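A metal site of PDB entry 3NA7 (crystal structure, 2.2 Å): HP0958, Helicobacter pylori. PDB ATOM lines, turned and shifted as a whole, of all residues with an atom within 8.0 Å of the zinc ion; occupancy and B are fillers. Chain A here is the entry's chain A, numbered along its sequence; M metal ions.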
ATOM      1  N   TRP A 187      -2.639  14.947  18.678  1.00  0.00           N
ATOM      2  CA  TRP A 187      -2.495  14.313  19.998  1.00  0.00           C
ATOM      3  C   TRP A 187      -3.828  13.875  20.621  1.00  0.00           C
ATOM      4  O   TRP A 187      -3.883  12.850  21.284  1.00  0.00           O
ATOM      5  CB  TRP A 187      -1.691  15.197  20.980  1.00  0.00           C
ATOM      6  CG  TRP A 187      -2.411  16.469  21.446  1.00  0.00           C
ATOM      7  CD1 TRP A 187      -2.304  17.719  20.897  1.00  0.00           C
ATOM      8  CD2 TRP A 187      -3.334  16.601  22.553  1.00  0.00           C
ATOM      9  NE1 TRP A 187      -3.101  18.611  21.588  1.00  0.00           N
ATOM     10  CE2 TRP A 187      -3.740  17.958  22.599  1.00  0.00           C
ATOM     11  CE3 TRP A 187      -3.854  15.705  23.501  1.00  0.00           C
ATOM     12  CZ2 TRP A 187      -4.644  18.431  23.555  1.00  0.00           C
ATOM     13  CZ3 TRP A 187      -4.742  16.193  24.459  1.00  0.00           C
ATOM     14  CH2 TRP A 187      -5.138  17.534  24.468  1.00  0.00           C
ATOM     15  N   THR A 191     -11.163  13.205  20.871  1.00  0.00           N
ATOM     16  CA  THR A 191     -11.531  14.014  22.021  1.00  0.00           C
ATOM     17  C   THR A 191     -11.065  15.455  21.785  1.00  0.00           C
ATOM     18  O   THR A 191     -10.823  16.192  22.743  1.00  0.00           O
ATOM     19  CB  THR A 191     -10.938  13.476  23.351  1.00  0.00           C
ATOM     20  OG1 THR A 191      -9.558  13.869  23.458  1.00  0.00           O
ATOM     21  CG2 THR A 191     -11.060  11.941  23.433  1.00  0.00           C
ATOM     22  N   VAL A 194     -14.772  19.065  22.707  1.00  0.00           N
ATOM     23  CA  VAL A 194     -15.571  18.558  23.825  1.00  0.00           C
ATOM     24  C   VAL A 194     -16.577  19.579  24.364  1.00  0.00           C
ATOM     25  O   VAL A 194     -16.355  20.782  24.285  1.00  0.00           O
ATOM     26  CB  VAL A 194     -14.672  18.027  24.944  1.00  0.00           C
ATOM     27  CG1 VAL A 194     -14.045  16.682  24.515  1.00  0.00           C
ATOM     28  CG2 VAL A 194     -13.594  19.066  25.330  1.00  0.00           C
ATOM     29  N   ALA A 200     -16.467  21.548  34.335  1.00  0.00           N
ATOM     30  CA  ALA A 200     -15.129  21.058  34.038  1.00  0.00           C
ATOM     31  C   ALA A 200     -14.956  20.752  32.543  1.00  0.00           C
ATOM     32  O   ALA A 200     -15.943  20.542  31.825  1.00  0.00           O
ATOM     33  CB  ALA A 200     -14.824  19.821  34.872  1.00  0.00           C
ATOM     34  N   CYS A 201     -13.709  20.728  32.077  1.00  0.00           N
ATOM     35  CA  CYS A 201     -13.440  20.410  30.672  1.00  0.00           C
ATOM     36  C   CYS A 201     -13.982  19.013  30.406  1.00  0.00           C
ATOM     37  O   CYS A 201     -13.676  18.101  31.163  1.00  0.00           O
ATOM     38  CB  CYS A 201     -11.928  20.463  30.406  1.00  0.00           C
ATOM     39  SG  CYS A 201     -11.337  19.854  28.764  1.00  0.00           S
ATOM     40  N   GLY A 202     -14.796  18.840  29.367  1.00  0.00           N
ATOM     41  CA  GLY A 202     -15.277  17.514  28.976  1.00  0.00           C
ATOM     42  C   GLY A 202     -14.194  16.543  28.496  1.00  0.00           C
ATOM     43  O   GLY A 202     -14.489  15.384  28.163  1.00  0.00           O
ATOM     44  N   GLY A 203     -12.955  17.028  28.448  1.00  0.00           N
ATOM     45  CA  GLY A 203     -11.810  16.259  27.974  1.00  0.00           C
ATOM     46  C   GLY A 203     -10.775  15.949  29.040  1.00  0.00           C
ATOM     47  O   GLY A 203     -10.285  14.843  29.098  1.00  0.00           O
ATOM     48  N   CYS A 204     -10.415  16.926  29.879  1.00  0.00           N
ATOM     49  CA  CYS A 204      -9.518  16.627  31.026  1.00  0.00           C
ATOM     50  C   CYS A 204     -10.200  16.601  32.400  1.00  0.00           C
ATOM     51  O   CYS A 204      -9.593  16.168  33.375  1.00  0.00           O
ATOM     52  CB  CYS A 204      -8.307  17.565  31.037  1.00  0.00           C
ATOM     53  SG  CYS A 204      -8.679  19.273  31.412  1.00  0.00           S
ATOM     54  N   PHE A 205     -11.448  17.077  32.473  1.00  0.00           N
ATOM     55  CA  PHE A 205     -12.317  16.988  33.662  1.00  0.00           C
ATOM     56  C   PHE A 205     -11.880  17.826  34.837  1.00  0.00           C
ATOM     57  O   PHE A 205     -12.317  17.625  35.957  1.00  0.00           O
ATOM     58  CB  PHE A 205     -12.577  15.527  34.073  1.00  0.00           C
ATOM     59  CG  PHE A 205     -12.980  14.647  32.925  1.00  0.00           C
ATOM     60  CD1 PHE A 205     -12.026  13.911  32.226  1.00  0.00           C
ATOM     61  CD2 PHE A 205     -14.315  14.555  32.536  1.00  0.00           C
ATOM     62  CE1 PHE A 205     -12.393  13.104  31.157  1.00  0.00           C
ATOM     63  CE2 PHE A 205     -14.688  13.749  31.454  1.00  0.00           C
ATOM     64  CZ  PHE A 205     -13.722  13.016  30.773  1.00  0.00           C
ATOM     65  N   ILE A 206     -11.032  18.809  34.580  1.00  0.00           N
ATOM     66  CA  ILE A 206     -10.589  19.732  35.616  1.00  0.00           C
ATOM     67  C   ILE A 206     -11.476  20.960  35.592  1.00  0.00           C
ATOM     68  O   ILE A 206     -11.773  21.490  34.531  1.00  0.00           O
ATOM     69  CB  ILE A 206      -9.095  20.092  35.410  1.00  0.00           C
ATOM     70  CG1 ILE A 206      -8.253  18.814  35.408  1.00  0.00           C
ATOM     71  CG2 ILE A 206      -8.621  21.098  36.466  1.00  0.00           C
ATOM     72  CD1 ILE A 206      -6.910  18.951  34.729  1.00  0.00           C
ATOM     73  N   ARG A 207     -11.931  21.398  36.765  1.00  0.00           N
ATOM     74  CA  ARG A 207     -12.965  22.437  36.856  1.00  0.00           C
ATOM     75  C   ARG A 207     -12.503  23.738  36.220  1.00  0.00           C
ATOM     76  O   ARG A 207     -11.382  24.182  36.440  1.00  0.00           O
ATOM     77  CB  ARG A 207     -13.352  22.672  38.323  1.00  0.00           C
ATOM     78  CG  ARG A 207     -14.796  23.099  38.534  1.00  0.00           C
ATOM     79  CD  ARG A 207     -15.728  21.872  38.758  1.00  0.00           C
ATOM     80  NE  ARG A 207     -16.226  21.724  40.140  1.00  0.00           N
ATOM     81  CZ  ARG A 207     -16.717  22.704  40.892  1.00  0.00           C
ATOM     82  NH1 ARG A 207     -16.775  23.954  40.450  1.00  0.00           N
ATOM     83  NH2 ARG A 207     -17.148  22.430  42.124  1.00  0.00           N
ATOM     84  N   LEU A 208     -13.358  24.342  35.391  1.00  0.00           N
ATOM     85  CA  LEU A 208     -13.021  25.601  34.733  1.00  0.00           C
ATOM     86  C   LEU A 208     -13.362  26.748  35.666  1.00  0.00           C
ATOM     87  O   LEU A 208     -14.393  26.685  36.332  1.00  0.00           O
ATOM     88  CB  LEU A 208     -13.806  25.734  33.426  1.00  0.00           C
ATOM     89  CG  LEU A 208     -13.526  24.625  32.391  1.00  0.00           C
ATOM     90  CD1 LEU A 208     -14.718  24.360  31.467  1.00  0.00           C
ATOM     91  CD2 LEU A 208     -12.278  24.973  31.600  1.00  0.00           C
ATOM     92  N   THR A 224     -10.510  27.324  23.902  1.00  0.00           N
ATOM     93  CA  THR A 224      -9.799  26.100  24.254  1.00  0.00           C
ATOM     94  C   THR A 224      -9.659  26.001  25.755  1.00  0.00           C
ATOM     95  O   THR A 224      -9.556  27.019  26.450  1.00  0.00           O
ATOM     96  CB  THR A 224      -8.384  26.019  23.650  1.00  0.00           C
ATOM     97  OG1 THR A 224      -7.545  27.040  24.203  1.00  0.00           O
ATOM     98  CG2 THR A 224      -8.430  26.113  22.140  1.00  0.00           C
ATOM     99  N   CYS A 225      -9.640  24.776  26.247  1.00  0.00           N
ATOM    100  CA  CYS A 225      -9.420  24.534  27.652  1.00  0.00           C
ATOM    101  C   CYS A 225      -8.011  24.973  28.037  1.00  0.00           C
ATOM    102  O   CYS A 225      -7.056  24.681  27.329  1.00  0.00           O
ATOM    103  CB  CYS A 225      -9.611  23.047  27.992  1.00  0.00           C
ATOM    104  SG  CYS A 225      -8.964  22.651  29.617  1.00  0.00           S
ATOM    105  N   PRO A 226      -7.888  25.672  29.171  1.00  0.00           N
ATOM    106  CA  PRO A 226      -6.565  26.174  29.560  1.00  0.00           C
ATOM    107  C   PRO A 226      -5.667  25.112  30.201  1.00  0.00           C
ATOM    108  O   PRO A 226      -4.467  25.356  30.395  1.00  0.00           O
ATOM    109  CB  PRO A 226      -6.910  27.282  30.553  1.00  0.00           C
ATOM    110  CG  PRO A 226      -8.198  26.820  31.193  1.00  0.00           C
ATOM    111  CD  PRO A 226      -8.952  26.102  30.095  1.00  0.00           C
ATOM    112  N   TYR A 227      -6.224  23.954  30.539  1.00  0.00           N
ATOM    113  CA  TYR A 227      -5.423  22.867  31.124  1.00  0.00           C
ATOM    114  C   TYR A 227      -4.866  21.910  30.094  1.00  0.00           C
ATOM    115  O   TYR A 227      -3.723  21.437  30.233  1.00  0.00           O
ATOM    116  CB  TYR A 227      -6.191  22.109  32.191  1.00  0.00           C
ATOM    117  CG  TYR A 227      -7.040  23.005  33.082  1.00  0.00           C
ATOM    118  CD1 TYR A 227      -6.461  24.011  33.864  1.00  0.00           C
ATOM    119  CD2 TYR A 227      -8.416  22.846  33.125  1.00  0.00           C
ATOM    120  CE1 TYR A 227      -7.230  24.834  34.674  1.00  0.00           C
ATOM    121  CE2 TYR A 227      -9.208  23.671  33.945  1.00  0.00           C
ATOM    122  CZ  TYR A 227      -8.608  24.658  34.716  1.00  0.00           C
ATOM    123  OH  TYR A 227      -9.380  25.464  35.525  1.00  0.00           O
ATOM    124  N   CYS A 228      -5.628  21.616  29.034  1.00  0.00           N
ATOM    125  CA  CYS A 228      -5.181  20.598  28.072  1.00  0.00           C
ATOM    126  C   CYS A 228      -5.163  21.013  26.613  1.00  0.00           C
ATOM    127  O   CYS A 228      -4.525  20.345  25.806  1.00  0.00           O
ATOM    128  CB  CYS A 228      -6.014  19.324  28.203  1.00  0.00           C
ATOM    129  SG  CYS A 228      -7.659  19.625  27.643  1.00  0.00           S
ATOM    130  N   GLY A 229      -5.857  22.078  26.242  1.00  0.00           N
ATOM    131  CA  GLY A 229      -5.720  22.645  24.906  1.00  0.00           C
ATOM    132  C   GLY A 229      -6.876  22.312  23.974  1.00  0.00           C
ATOM    133  O   GLY A 229      -6.952  22.836  22.867  1.00  0.00           O
ATOM    134  N   ARG A 230      -7.776  21.433  24.419  1.00  0.00           N
ATOM    135  CA  ARG A 230      -8.928  21.044  23.626  1.00  0.00           C
ATOM    136  C   ARG A 230      -9.863  22.234  23.301  1.00  0.00           C
ATOM    137  O   ARG A 230      -9.882  23.229  24.029  1.00  0.00           O
ATOM    138  CB  ARG A 230      -9.699  19.948  24.368  1.00  0.00           C
ATOM    139  CG  ARG A 230      -8.941  18.631  24.474  1.00  0.00           C
ATOM    140  CD  ARG A 230      -9.717  17.608  25.273  1.00  0.00           C
ATOM    141  NE  ARG A 230      -9.154  16.268  25.134  1.00  0.00           N
ATOM    142  CZ  ARG A 230      -8.287  15.725  25.988  1.00  0.00           C
ATOM    143  NH1 ARG A 230      -7.895  16.401  27.061  1.00  0.00           N
ATOM    144  NH2 ARG A 230      -7.823  14.506  25.780  1.00  0.00           N
ATOM    145  N   ILE A 231     -10.629  22.105  22.217  1.00  0.00           N
ATOM    146  CA  ILE A 231     -11.709  23.020  21.912  1.00  0.00           C
ATOM    147  C   ILE A 231     -12.935  22.698  22.782  1.00  0.00           C
ATOM    148  O   ILE A 231     -13.323  21.529  22.903  1.00  0.00           O
ATOM    149  CB  ILE A 231     -12.094  22.960  20.424  1.00  0.00           C
ATOM    150  CG1 ILE A 231     -10.930  23.396  19.539  1.00  0.00           C
ATOM    151  CG2 ILE A 231     -13.327  23.833  20.154  1.00  0.00           C
ATOM    152  CD1 ILE A 231     -11.053  22.911  18.107  1.00  0.00           C
ATOM    153  N   LEU A 232     -13.532  23.743  23.355  1.00  0.00           N
ATOM    154  CA  LEU A 232     -14.689  23.650  24.254  1.00  0.00           C
ATOM    155  C   LEU A 232     -15.924  24.383  23.730  1.00  0.00           C
ATOM    156  O   LEU A 232     -15.816  25.475  23.185  1.00  0.00           O
ATOM    157  CB  LEU A 232     -14.356  24.255  25.621  1.00  0.00           C
ATOM    158  CG  LEU A 232     -13.755  23.389  26.716  1.00  0.00           C
ATOM    159  CD1 LEU A 232     -13.419  24.285  27.901  1.00  0.00           C
ATOM    160  CD2 LEU A 232     -14.707  22.292  27.118  1.00  0.00           C
HETATM  161 ZN    ZN M   1      -9.331  20.208  29.345  1.00  0.00          ZN
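The backbone NH (N) of Gly 203 lies close to the side-chain sulfur (SG) of Cys 201 (3.3 Å).
N of Cys 201 sits at hydrogen-bond distance from O of Ile 206 (3.2 Å).
The side-chain sulfur (SG) of Cys 228 lies close to the guanidinium group (NH1) of Arg 230.
The side-chain sulfur of Cys 225 sits close to the backbone NH of Tyr 227.
The backbone NH (N) of Cys 225 is in hydrogen-bond range of the backbone carbonyl oxygen (O) of Arg 230 (2.7 Å).
The zinc ion is bound by SG of Cys 201, SG of Cys 204, SG of Cys 228 and SG of Cys 225.
The zinc ion has four donor atoms within binding distance.
Four residues have an atom within 4 Å of the zinc ion: Cys 201, Cys 204, Cys 225 and Cys 228.
The nearest printed residue that does not touch the zinc ion is Gly 203 (4.5 Å).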
